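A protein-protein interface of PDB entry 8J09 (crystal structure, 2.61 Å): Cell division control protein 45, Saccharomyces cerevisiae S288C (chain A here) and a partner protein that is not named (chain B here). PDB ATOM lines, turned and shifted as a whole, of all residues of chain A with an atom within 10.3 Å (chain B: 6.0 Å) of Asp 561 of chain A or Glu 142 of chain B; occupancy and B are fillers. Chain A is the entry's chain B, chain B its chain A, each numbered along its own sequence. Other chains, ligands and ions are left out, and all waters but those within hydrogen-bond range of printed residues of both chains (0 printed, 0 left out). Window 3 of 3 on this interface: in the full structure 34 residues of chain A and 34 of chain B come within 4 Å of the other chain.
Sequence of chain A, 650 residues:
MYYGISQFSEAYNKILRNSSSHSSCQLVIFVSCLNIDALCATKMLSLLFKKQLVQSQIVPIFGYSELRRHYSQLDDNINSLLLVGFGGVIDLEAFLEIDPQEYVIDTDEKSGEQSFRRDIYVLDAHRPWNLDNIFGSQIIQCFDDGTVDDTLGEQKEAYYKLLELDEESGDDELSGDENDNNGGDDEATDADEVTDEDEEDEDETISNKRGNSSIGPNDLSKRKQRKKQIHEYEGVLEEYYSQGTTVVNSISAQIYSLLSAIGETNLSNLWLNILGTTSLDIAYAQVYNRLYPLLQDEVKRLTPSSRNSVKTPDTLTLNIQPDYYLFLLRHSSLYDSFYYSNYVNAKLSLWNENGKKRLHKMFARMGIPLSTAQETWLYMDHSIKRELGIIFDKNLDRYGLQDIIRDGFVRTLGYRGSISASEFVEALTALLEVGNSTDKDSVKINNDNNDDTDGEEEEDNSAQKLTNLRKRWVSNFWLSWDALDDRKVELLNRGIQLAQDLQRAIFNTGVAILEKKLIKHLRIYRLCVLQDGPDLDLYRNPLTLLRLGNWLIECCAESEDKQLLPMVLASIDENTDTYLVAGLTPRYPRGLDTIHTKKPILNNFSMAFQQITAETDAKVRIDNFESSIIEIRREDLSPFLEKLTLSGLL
OE1 of Glu 142 of chain B sits close to O of Asp 561 of chain A, 3.1 Å away.
Printed residues of chain B within 4 Å of His 521 of chain A: Pro 267.
Asp 561 of chain A touches just one residue of chain B: Glu 142 (3.1 Å).
Glu 142 of chain B touches just one residue of chain A: Asp 561.
Of the printed residues of chain A, Lys 146 of chain B touches Ile 601 (3.6 Å).
Printed residues of chain A within 4 Å of Phe 259 of chain B: Arg 523 (3.6 Å).
Of the printed residues of chain A, Pro 267 of chain B touches His 521 and Lys 562.
The nearest residue of chain A that does not touch Glu 142 of chain B is Arg 523 of chain A (4.1 Å).
The nearest printed residue of chain B that does not touch Lys 562 of chain A is Glu 142 of chain B (5.2 Å).
A ring nitrogen (ND1) of His 521 of chain A lies close to the side-chain amino group (NZ) of Lys 562 of chain A, at 3.3 Å.
His 521 of chain A touches Pro 267 of chain B (CD2 to CD, 3.5 Å).
CD2 of Phe 141 of chain B touches NH2 of Arg 523 of chain A (3.6 Å).
CG of Arg 523 of chain A touches CE2 of Tyr 145 of chain B (3.9 Å).
Phe 259 of chain B touches Arg 523 of chain A (CE1 to NH2, 3.6 Å).
Pro 267 of chain B touches Lys 562 of chain A (CG to CE, 3.6 Å).
CG2 of Ile 601 of chain A touches O of Lys 146 of chain B, 3.6 Å away.
Hydrophobic or aromatic side chains of chain B within 4 Å of the printed part of chain A: Phe 141, Tyr 145, Phe 259 and Pro 267.
Of the 23 printed residues of chain A, 5 touch a printed residue of chain B.
Printed residues of chain A that touch a printed residue of chain B: His 521, Arg 523, Asp 561, Lys 562 and Ile 601.
Along chain A the printed residues that touch a printed residue of chain B span positions 521 to 601.
Among the printed residues, no Asp or Glu carboxylate lies within 4 Å of a Lys or Arg side-chain nitrogen of the other chain.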
ATOM      1  N   HIS A 521     -24.979  16.513  19.780  1.00  0.00           N
ATOM      2  CA  HIS A 521     -24.685  15.959  18.462  1.00  0.00           C
ATOM      3  C   HIS A 521     -23.700  14.804  18.574  1.00  0.00           C
ATOM      4  O   HIS A 521     -22.533  15.003  18.925  1.00  0.00           O
ATOM      5  CB  HIS A 521     -24.150  17.054  17.532  1.00  0.00           C
ATOM      6  CG  HIS A 521     -25.068  18.230  17.402  1.00  0.00           C
ATOM      7  ND1 HIS A 521     -26.301  18.145  16.794  1.00  0.00           N
ATOM      8  CD2 HIS A 521     -24.929  19.521  17.788  1.00  0.00           C
ATOM      9  CE1 HIS A 521     -26.893  19.326  16.832  1.00  0.00           C
ATOM     10  NE2 HIS A 521     -26.080  20.179  17.428  1.00  0.00           N
ATOM     11  N   LEU A 522     -24.170  13.605  18.254  1.00  0.00           N
ATOM     12  CA  LEU A 522     -23.351  12.408  18.246  1.00  0.00           C
ATOM     13  C   LEU A 522     -23.006  12.046  16.801  1.00  0.00           C
ATOM     14  O   LEU A 522     -23.397  12.732  15.853  1.00  0.00           O
ATOM     15  CB  LEU A 522     -24.072  11.268  18.970  1.00  0.00           C
ATOM     16  CG  LEU A 522     -24.117  11.312  20.505  1.00  0.00           C
ATOM     17  CD1 LEU A 522     -24.946  12.473  21.041  1.00  0.00           C
ATOM     18  CD2 LEU A 522     -24.653  10.003  21.046  1.00  0.00           C
ATOM     19  N   ARG A 523     -22.263  10.950  16.633  1.00  0.00           N
ATOM     20  CA  ARG A 523     -21.725  10.618  15.316  1.00  0.00           C
ATOM     21  C   ARG A 523     -22.834  10.307  14.316  1.00  0.00           C
ATOM     22  O   ARG A 523     -22.828  10.818  13.190  1.00  0.00           O
ATOM     23  CB  ARG A 523     -20.757   9.440  15.424  1.00  0.00           C
ATOM     24  CG  ARG A 523     -20.144   9.022  14.094  1.00  0.00           C
ATOM     25  CD  ARG A 523     -19.544  10.215  13.357  1.00  0.00           C
ATOM     26  NE  ARG A 523     -18.501  10.872  14.140  1.00  0.00           N
ATOM     27  CZ  ARG A 523     -18.153  12.147  13.999  1.00  0.00           C
ATOM     28  NH1 ARG A 523     -18.764  12.909  13.102  1.00  0.00           N
ATOM     29  NH2 ARG A 523     -17.194  12.661  14.758  1.00  0.00           N
ATOM     30  N   ILE A 524     -23.797   9.474  14.705  1.00  0.00           N
ATOM     31  CA  ILE A 524     -24.808   8.986  13.774  1.00  0.00           C
ATOM     32  C   ILE A 524     -26.198   9.522  14.071  1.00  0.00           C
ATOM     33  O   ILE A 524     -27.128   9.244  13.299  1.00  0.00           O
ATOM     34  CB  ILE A 524     -24.832   7.447  13.726  1.00  0.00           C
ATOM     35  CG1 ILE A 524     -25.412   6.877  15.020  1.00  0.00           C
ATOM     36  CG2 ILE A 524     -23.436   6.900  13.465  1.00  0.00           C
ATOM     37  CD1 ILE A 524     -26.145   5.575  14.824  1.00  0.00           C
ATOM     38  N   TYR A 525     -26.381  10.280  15.151  1.00  0.00           N
ATOM     39  CA  TYR A 525     -27.690  10.855  15.427  1.00  0.00           C
ATOM     40  C   TYR A 525     -27.541  12.042  16.365  1.00  0.00           C
ATOM     41  O   TYR A 525     -26.524  12.201  17.045  1.00  0.00           O
ATOM     42  CB  TYR A 525     -28.655   9.815  16.018  1.00  0.00           C
ATOM     43  CG  TYR A 525     -28.319   9.342  17.420  1.00  0.00           C
ATOM     44  CD1 TYR A 525     -28.840   9.983  18.537  1.00  0.00           C
ATOM     45  CD2 TYR A 525     -27.498   8.240  17.622  1.00  0.00           C
ATOM     46  CE1 TYR A 525     -28.543   9.549  19.813  1.00  0.00           C
ATOM     47  CE2 TYR A 525     -27.195   7.797  18.897  1.00  0.00           C
ATOM     48  CZ  TYR A 525     -27.721   8.456  19.988  1.00  0.00           C
ATOM     49  OH  TYR A 525     -27.423   8.022  21.259  1.00  0.00           O
ATOM     50  N   ARG A 526     -28.576  12.874  16.387  1.00  0.00           N
ATOM     51  CA  ARG A 526     -28.665  13.997  17.306  1.00  0.00           C
ATOM     52  C   ARG A 526     -29.601  13.647  18.453  1.00  0.00           C
ATOM     53  O   ARG A 526     -30.636  13.006  18.252  1.00  0.00           O
ATOM     54  CB  ARG A 526     -29.157  15.249  16.588  1.00  0.00           C
ATOM     55  CG  ARG A 526     -28.262  15.665  15.450  1.00  0.00           C
ATOM     56  CD  ARG A 526     -28.892  16.795  14.690  1.00  0.00           C
ATOM     57  NE  ARG A 526     -29.956  16.319  13.816  1.00  0.00           N
ATOM     58  CZ  ARG A 526     -30.737  17.119  13.100  1.00  0.00           C
ATOM     59  NH1 ARG A 526     -30.567  18.430  13.165  1.00  0.00           N
ATOM     60  NH2 ARG A 526     -31.685  16.614  12.323  1.00  0.00           N
ATOM     61  N   CYS A 556     -34.459  24.477  12.884  1.00  0.00           N
ATOM     62  CA  CYS A 556     -33.115  24.731  13.381  1.00  0.00           C
ATOM     63  C   CYS A 556     -32.149  24.920  12.219  1.00  0.00           C
ATOM     64  O   CYS A 556     -32.336  24.371  11.130  1.00  0.00           O
ATOM     65  CB  CYS A 556     -32.641  23.584  14.275  1.00  0.00           C
ATOM     66  SG  CYS A 556     -31.838  22.227  13.390  1.00  0.00           S
ATOM     67  N   ALA A 557     -31.110  25.721  12.457  1.00  0.00           N
ATOM     68  CA  ALA A 557     -30.071  25.926  11.455  1.00  0.00           C
ATOM     69  C   ALA A 557     -29.172  24.698  11.375  1.00  0.00           C
ATOM     70  O   ALA A 557     -29.329  23.867  10.475  1.00  0.00           O
ATOM     71  CB  ALA A 557     -29.253  27.179  11.776  1.00  0.00           C
ATOM     72  N   GLU A 558     -28.231  24.585  12.315  1.00  0.00           N
ATOM     73  CA  GLU A 558     -27.391  23.396  12.491  1.00  0.00           C
ATOM     74  C   GLU A 558     -26.617  23.060  11.216  1.00  0.00           C
ATOM     75  O   GLU A 558     -26.450  21.892  10.847  1.00  0.00           O
ATOM     76  CB  GLU A 558     -28.210  22.201  12.973  1.00  0.00           C
ATOM     77  CG  GLU A 558     -28.013  21.899  14.459  1.00  0.00           C
ATOM     78  CD  GLU A 558     -29.010  20.889  14.998  1.00  0.00           C
ATOM     79  OE1 GLU A 558     -29.442  21.039  16.161  1.00  0.00           O
ATOM     80  OE2 GLU A 558     -29.360  19.942  14.262  1.00  0.00           O
ATOM     81  N   SER A 559     -26.155  24.102  10.535  1.00  0.00           N
ATOM     82  CA  SER A 559     -25.072  24.021   9.542  1.00  0.00           C
ATOM     83  C   SER A 559     -25.536  23.166   8.354  1.00  0.00           C
ATOM     84  O   SER A 559     -26.673  23.327   7.881  1.00  0.00           O
ATOM     85  CB  SER A 559     -23.809  23.543  10.237  1.00  0.00           C
ATOM     86  OG  SER A 559     -23.180  24.602  10.947  1.00  0.00           O
ATOM     87  N   GLU A 560     -24.675  22.281   7.850  1.00  0.00           N
ATOM     88  CA  GLU A 560     -24.859  21.537   6.611  1.00  0.00           C
ATOM     89  C   GLU A 560     -24.565  20.070   6.893  1.00  0.00           C
ATOM     90  O   GLU A 560     -25.370  19.174   6.621  1.00  0.00           O
ATOM     91  CB  GLU A 560     -23.912  22.059   5.521  1.00  0.00           C
ATOM     92  CG  GLU A 560     -23.714  23.590   5.466  1.00  0.00           C
ATOM     93  CD  GLU A 560     -22.823  24.150   6.583  1.00  0.00           C
ATOM     94  OE1 GLU A 560     -23.116  25.267   7.062  1.00  0.00           O
ATOM     95  OE2 GLU A 560     -21.850  23.478   6.990  1.00  0.00           O
ATOM     96  N   ASP A 561     -23.394  19.841   7.469  1.00  0.00           N
ATOM     97  CA  ASP A 561     -22.893  18.532   7.862  1.00  0.00           C
ATOM     98  C   ASP A 561     -23.799  17.790   8.840  1.00  0.00           C
ATOM     99  O   ASP A 561     -23.486  16.660   9.226  1.00  0.00           O
ATOM    100  CB  ASP A 561     -21.523  18.712   8.504  1.00  0.00           C
ATOM    101  CG  ASP A 561     -21.558  19.726   9.629  1.00  0.00           C
ATOM    102  OD1 ASP A 561     -20.657  19.703  10.490  1.00  0.00           O
ATOM    103  OD2 ASP A 561     -22.508  20.539   9.652  1.00  0.00           O
ATOM    104  N   LYS A 562     -24.909  18.396   9.262  1.00  0.00           N
ATOM    105  CA  LYS A 562     -25.512  17.969  10.519  1.00  0.00           C
ATOM    106  C   LYS A 562     -27.014  17.717  10.471  1.00  0.00           C
ATOM    107  O   LYS A 562     -27.514  16.841  11.182  1.00  0.00           O
ATOM    108  CB  LYS A 562     -25.205  19.014  11.589  1.00  0.00           C
ATOM    109  CG  LYS A 562     -25.843  18.758  12.917  1.00  0.00           C
ATOM    110  CD  LYS A 562     -24.976  19.410  13.947  1.00  0.00           C
ATOM    111  CE  LYS A 562     -23.847  18.473  14.292  1.00  0.00           C
ATOM    112  NZ  LYS A 562     -24.369  17.080  14.277  1.00  0.00           N
ATOM    113  N   GLN A 563     -27.753  18.480   9.667  1.00  0.00           N
ATOM    114  CA  GLN A 563     -29.183  18.225   9.589  1.00  0.00           C
ATOM    115  C   GLN A 563     -29.488  16.965   8.790  1.00  0.00           C
ATOM    116  O   GLN A 563     -30.583  16.413   8.921  1.00  0.00           O
ATOM    117  CB  GLN A 563     -29.920  19.441   9.006  1.00  0.00           C
ATOM    118  CG  GLN A 563     -31.447  19.353   9.136  1.00  0.00           C
ATOM    119  CD  GLN A 563     -31.933  19.497  10.576  1.00  0.00           C
ATOM    120  OE1 GLN A 563     -32.484  18.563  11.157  1.00  0.00           O
ATOM    121  NE2 GLN A 563     -31.728  20.673  11.153  1.00  0.00           N
ATOM    122  N   LEU A 564     -28.527  16.464   8.016  1.00  0.00           N
ATOM    123  CA  LEU A 564     -28.655  15.129   7.446  1.00  0.00           C
ATOM    124  C   LEU A 564     -28.723  14.049   8.517  1.00  0.00           C
ATOM    125  O   LEU A 564     -29.065  12.905   8.199  1.00  0.00           O
ATOM    126  CB  LEU A 564     -27.482  14.837   6.502  1.00  0.00           C
ATOM    127  CG  LEU A 564     -27.480  15.495   5.120  1.00  0.00           C
ATOM    128  CD1 LEU A 564     -26.245  15.076   4.331  1.00  0.00           C
ATOM    129  CD2 LEU A 564     -28.748  15.151   4.353  1.00  0.00           C
ATOM    130  N   LEU A 565     -28.408  14.384   9.774  1.00  0.00           N
ATOM    131  CA  LEU A 565     -28.397  13.423  10.865  1.00  0.00           C
ATOM    132  C   LEU A 565     -29.810  13.206  11.400  1.00  0.00           C
ATOM    133  O   LEU A 565     -30.598  14.152  11.474  1.00  0.00           O
ATOM    134  CB  LEU A 565     -27.498  13.903  12.003  1.00  0.00           C
ATOM    135  CG  LEU A 565     -25.988  13.933  11.775  1.00  0.00           C
ATOM    136  CD1 LEU A 565     -25.257  13.942  13.108  1.00  0.00           C
ATOM    137  CD2 LEU A 565     -25.550  12.752  10.924  1.00  0.00           C
ATOM    138  N   PRO A 566     -30.147  11.978  11.776  1.00  0.00           N
ATOM    139  CA  PRO A 566     -31.417  11.737  12.464  1.00  0.00           C
ATOM    140  C   PRO A 566     -31.415  12.367  13.848  1.00  0.00           C
ATOM    141  O   PRO A 566     -30.373  12.718  14.403  1.00  0.00           O
ATOM    142  CB  PRO A 566     -31.494  10.208  12.554  1.00  0.00           C
ATOM    143  CG  PRO A 566     -30.465   9.700  11.581  1.00  0.00           C
ATOM    144  CD  PRO A 566     -29.398  10.735  11.539  1.00  0.00           C
ATOM    145  N   PRO A 586     -34.766  12.960   8.909  1.00  0.00           N
ATOM    146  CA  PRO A 586     -35.147  14.211   8.239  1.00  0.00           C
ATOM    147  C   PRO A 586     -35.733  13.936   6.861  1.00  0.00           C
ATOM    148  O   PRO A 586     -35.209  13.125   6.095  1.00  0.00           O
ATOM    149  CB  PRO A 586     -33.825  14.982   8.148  1.00  0.00           C
ATOM    150  CG  PRO A 586     -32.953  14.375   9.202  1.00  0.00           C
ATOM    151  CD  PRO A 586     -33.337  12.930   9.259  1.00  0.00           C
ATOM    152  N   THR A 597     -27.086  18.386  -3.126  1.00  0.00           N
ATOM    153  CA  THR A 597     -27.010  17.729  -1.833  1.00  0.00           C
ATOM    154  C   THR A 597     -27.251  16.230  -1.984  1.00  0.00           C
ATOM    155  O   THR A 597     -27.861  15.758  -2.948  1.00  0.00           O
ATOM    156  CB  THR A 597     -28.021  18.327  -0.855  1.00  0.00           C
ATOM    157  OG1 THR A 597     -29.340  17.883  -1.193  1.00  0.00           O
ATOM    158  CG2 THR A 597     -27.972  19.847  -0.898  1.00  0.00           C
ATOM    159  N   LYS A 598     -26.756  15.480  -1.009  1.00  0.00           N
ATOM    160  CA  LYS A 598     -26.741  14.031  -1.071  1.00  0.00           C
ATOM    161  C   LYS A 598     -27.608  13.445   0.032  1.00  0.00           C
ATOM    162  O   LYS A 598     -27.769  14.042   1.103  1.00  0.00           O
ATOM    163  CB  LYS A 598     -25.310  13.499  -0.946  1.00  0.00           C
ATOM    164  CG  LYS A 598     -24.308  14.231  -1.824  1.00  0.00           C
ATOM    165  CD  LYS A 598     -24.277  13.625  -3.212  1.00  0.00           C
ATOM    166  CE  LYS A 598     -23.900  12.155  -3.142  1.00  0.00           C
ATOM    167  NZ  LYS A 598     -23.825  11.532  -4.491  1.00  0.00           N
ATOM    168  N   LYS A 599     -28.174  12.276  -0.244  1.00  0.00           N
ATOM    169  CA  LYS A 599     -28.843  11.521   0.799  1.00  0.00           C
ATOM    170  C   LYS A 599     -27.838  11.168   1.893  1.00  0.00           C
ATOM    171  O   LYS A 599     -26.660  10.927   1.597  1.00  0.00           O
ATOM    172  CB  LYS A 599     -29.464  10.242   0.230  1.00  0.00           C
ATOM    173  CG  LYS A 599     -30.856  10.412  -0.353  1.00  0.00           C
ATOM    174  CD  LYS A 599     -31.403   9.076  -0.831  1.00  0.00           C
ATOM    175  CE  LYS A 599     -32.746   9.238  -1.523  1.00  0.00           C
ATOM    176  NZ  LYS A 599     -33.793   9.747  -0.594  1.00  0.00           N
ATOM    177  N   PRO A 600     -28.253  11.144   3.158  1.00  0.00           N
ATOM    178  CA  PRO A 600     -27.334  10.714   4.218  1.00  0.00           C
ATOM    179  C   PRO A 600     -26.812   9.312   3.940  1.00  0.00           C
ATOM    180  O   PRO A 600     -27.557   8.427   3.513  1.00  0.00           O
ATOM    181  CB  PRO A 600     -28.198  10.761   5.486  1.00  0.00           C
ATOM    182  CG  PRO A 600     -29.618  10.797   4.999  1.00  0.00           C
ATOM    183  CD  PRO A 600     -29.580  11.509   3.685  1.00  0.00           C
ATOM    184  N   ILE A 601     -25.508   9.130   4.163  1.00  0.00           N
ATOM    185  CA  ILE A 601     -24.864   7.854   3.858  1.00  0.00           C
ATOM    186  C   ILE A 601     -25.541   6.720   4.614  1.00  0.00           C
ATOM    187  O   ILE A 601     -25.734   5.622   4.077  1.00  0.00           O
ATOM    188  CB  ILE A 601     -23.358   7.929   4.172  1.00  0.00           C
ATOM    189  CG1 ILE A 601     -22.676   8.952   3.260  1.00  0.00           C
ATOM    190  CG2 ILE A 601     -22.708   6.565   4.010  1.00  0.00           C
ATOM    191  CD1 ILE A 601     -22.659   8.554   1.797  1.00  0.00           C
ATOM    192  N   ARG B 139      -8.391  15.585  11.055  1.00  0.00           N
ATOM    193  CA  ARG B 139      -8.576  16.873  10.389  1.00  0.00           C
ATOM    194  C   ARG B 139     -10.015  17.025   9.908  1.00  0.00           C
ATOM    195  O   ARG B 139     -10.795  17.803  10.466  1.00  0.00           O
ATOM    196  CB  ARG B 139      -7.584  17.018   9.234  1.00  0.00           C
ATOM    197  CG  ARG B 139      -6.510  18.044   9.505  1.00  0.00           C
ATOM    198  CD  ARG B 139      -7.058  19.455   9.404  1.00  0.00           C
ATOM    199  NE  ARG B 139      -7.563  19.749   8.066  1.00  0.00           N
ATOM    200  CZ  ARG B 139      -8.046  20.929   7.696  1.00  0.00           C
ATOM    201  NH1 ARG B 139      -8.088  21.930   8.565  1.00  0.00           N
ATOM    202  NH2 ARG B 139      -8.483  21.110   6.456  1.00  0.00           N
ATOM    203  N   ASP B 140     -10.378  16.288   8.860  1.00  0.00           N
ATOM    204  CA  ASP B 140     -11.769  16.222   8.432  1.00  0.00           C
ATOM    205  C   ASP B 140     -12.320  14.840   8.752  1.00  0.00           C
ATOM    206  O   ASP B 140     -12.714  14.098   7.847  1.00  0.00           O
ATOM    207  CB  ASP B 140     -11.898  16.532   6.940  1.00  0.00           C
ATOM    208  CG  ASP B 140     -11.613  17.988   6.621  1.00  0.00           C
ATOM    209  OD1 ASP B 140     -12.348  18.864   7.126  1.00  0.00           O
ATOM    210  OD2 ASP B 140     -10.651  18.255   5.869  1.00  0.00           O
ATOM    211  N   PHE B 141     -12.334  14.492  10.043  1.00  0.00           N
ATOM    212  CA  PHE B 141     -12.760  13.159  10.460  1.00  0.00           C
ATOM    213  C   PHE B 141     -14.164  12.844   9.962  1.00  0.00           C
ATOM    214  O   PHE B 141     -14.452  11.705   9.576  1.00  0.00           O
ATOM    215  CB  PHE B 141     -12.692  13.048  11.985  1.00  0.00           C
ATOM    216  CG  PHE B 141     -13.081  11.696  12.517  1.00  0.00           C
ATOM    217  CD1 PHE B 141     -12.139  10.686  12.634  1.00  0.00           C
ATOM    218  CD2 PHE B 141     -14.386  11.440  12.911  1.00  0.00           C
ATOM    219  CE1 PHE B 141     -12.493   9.440  13.126  1.00  0.00           C
ATOM    220  CE2 PHE B 141     -14.747  10.198  13.403  1.00  0.00           C
ATOM    221  CZ  PHE B 141     -13.798   9.196  13.512  1.00  0.00           C
ATOM    222  N   GLU B 142     -15.050  13.842   9.959  1.00  0.00           N
ATOM    223  CA  GLU B 142     -16.411  13.625   9.480  1.00  0.00           C
ATOM    224  C   GLU B 142     -16.424  13.238   8.008  1.00  0.00           C
ATOM    225  O   GLU B 142     -17.245  12.417   7.580  1.00  0.00           O
ATOM    226  CB  GLU B 142     -17.247  14.885   9.711  1.00  0.00           C
ATOM    227  CG  GLU B 142     -18.694  14.776   9.257  1.00  0.00           C
ATOM    228  CD  GLU B 142     -19.638  15.599  10.115  1.00  0.00           C
ATOM    229  OE1 GLU B 142     -20.855  15.320  10.100  1.00  0.00           O
ATOM    230  OE2 GLU B 142     -19.162  16.524  10.807  1.00  0.00           O
ATOM    231  N   LYS B 143     -15.516  13.812   7.216  1.00  0.00           N
ATOM    232  CA  LYS B 143     -15.509  13.555   5.782  1.00  0.00           C
ATOM    233  C   LYS B 143     -14.849  12.226   5.435  1.00  0.00           C
ATOM    234  O   LYS B 143     -15.249  11.579   4.461  1.00  0.00           O
ATOM    235  CB  LYS B 143     -14.814  14.706   5.054  1.00  0.00           C
ATOM    236  CG  LYS B 143     -15.481  16.053   5.286  1.00  0.00           C
ATOM    237  CD  LYS B 143     -14.713  17.184   4.626  1.00  0.00           C
ATOM    238  CE  LYS B 143     -15.392  18.523   4.874  1.00  0.00           C
ATOM    239  NZ  LYS B 143     -14.635  19.653   4.264  1.00  0.00           N
ATOM    240  N   LYS B 144     -13.847  11.803   6.207  1.00  0.00           N
ATOM    241  CA  LYS B 144     -13.227  10.508   5.953  1.00  0.00           C
ATOM    242  C   LYS B 144     -14.114   9.363   6.423  1.00  0.00           C
ATOM    243  O   LYS B 144     -14.123   8.292   5.805  1.00  0.00           O
ATOM    244  CB  LYS B 144     -11.861  10.430   6.639  1.00  0.00           C
ATOM    245  CG  LYS B 144     -11.004  11.677   6.482  1.00  0.00           C
ATOM    246  CD  LYS B 144      -9.583  11.436   6.978  1.00  0.00           C
ATOM    247  CE  LYS B 144      -8.660  12.596   6.622  1.00  0.00           C
ATOM    248  NZ  LYS B 144      -8.791  13.738   7.571  1.00  0.00           N
ATOM    249  N   TYR B 145     -14.871   9.571   7.503  1.00  0.00           N
ATOM    250  CA  TYR B 145     -15.666   8.511   8.110  1.00  0.00           C
ATOM    251  C   TYR B 145     -16.847   8.073   7.252  1.00  0.00           C
ATOM    252  O   TYR B 145     -17.476   7.059   7.573  1.00  0.00           O
ATOM    253  CB  TYR B 145     -16.169   8.965   9.482  1.00  0.00           C
ATOM    254  CG  TYR B 145     -16.682   7.843  10.353  1.00  0.00           C
ATOM    255  CD1 TYR B 145     -15.809   6.930  10.928  1.00  0.00           C
ATOM    256  CD2 TYR B 145     -18.041   7.699  10.603  1.00  0.00           C
ATOM    257  CE1 TYR B 145     -16.273   5.901  11.727  1.00  0.00           C
ATOM    258  CE2 TYR B 145     -18.515   6.675  11.401  1.00  0.00           C
ATOM    259  CZ  TYR B 145     -17.627   5.779  11.961  1.00  0.00           C
ATOM    260  OH  TYR B 145     -18.095   4.757  12.756  1.00  0.00           O
ATOM    261  N   LYS B 146     -17.160   8.798   6.175  1.00  0.00           N
ATOM    262  CA  LYS B 146     -18.302   8.441   5.343  1.00  0.00           C
ATOM    263  C   LYS B 146     -18.152   7.066   4.703  1.00  0.00           C
ATOM    264  O   LYS B 146     -19.161   6.454   4.335  1.00  0.00           O
ATOM    265  CB  LYS B 146     -18.512   9.506   4.267  1.00  0.00           C
ATOM    266  CG  LYS B 146     -19.149  10.783   4.790  1.00  0.00           C
ATOM    267  CD  LYS B 146     -19.089  11.898   3.762  1.00  0.00           C
ATOM    268  CE  LYS B 146     -20.139  12.962   4.040  1.00  0.00           C
ATOM    269  NZ  LYS B 146     -19.923  14.183   3.215  1.00  0.00           N
ATOM    270  N   PHE B 259     -10.100  17.969  17.556  1.00  0.00           N
ATOM    271  CA  PHE B 259     -11.260  17.140  17.247  1.00  0.00           C
ATOM    272  C   PHE B 259     -12.101  16.885  18.492  1.00  0.00           C
ATOM    273  O   PHE B 259     -13.334  16.974  18.448  1.00  0.00           O
ATOM    274  CB  PHE B 259     -10.801  15.822  16.619  1.00  0.00           C
ATOM    275  CG  PHE B 259     -11.874  14.772  16.550  1.00  0.00           C
ATOM    276  CD1 PHE B 259     -12.829  14.803  15.547  1.00  0.00           C
ATOM    277  CD2 PHE B 259     -11.920  13.746  17.481  1.00  0.00           C
ATOM    278  CE1 PHE B 259     -13.815  13.835  15.477  1.00  0.00           C
ATOM    279  CE2 PHE B 259     -12.904  12.774  17.415  1.00  0.00           C
ATOM    280  CZ  PHE B 259     -13.852  12.820  16.412  1.00  0.00           C
ATOM    281  N   PRO B 267     -21.284  22.299  17.720  1.00  0.00           N
ATOM    282  CA  PRO B 267     -21.460  23.377  16.742  1.00  0.00           C
ATOM    283  C   PRO B 267     -22.591  24.331  17.117  1.00  0.00           C
ATOM    284  O   PRO B 267     -23.301  24.066  18.089  1.00  0.00           O
ATOM    285  CB  PRO B 267     -21.790  22.623  15.453  1.00  0.00           C
ATOM    286  CG  PRO B 267     -22.485  21.393  15.924  1.00  0.00           C
ATOM    287  CD  PRO B 267     -21.842  21.023  17.240  1.00  0.00           C
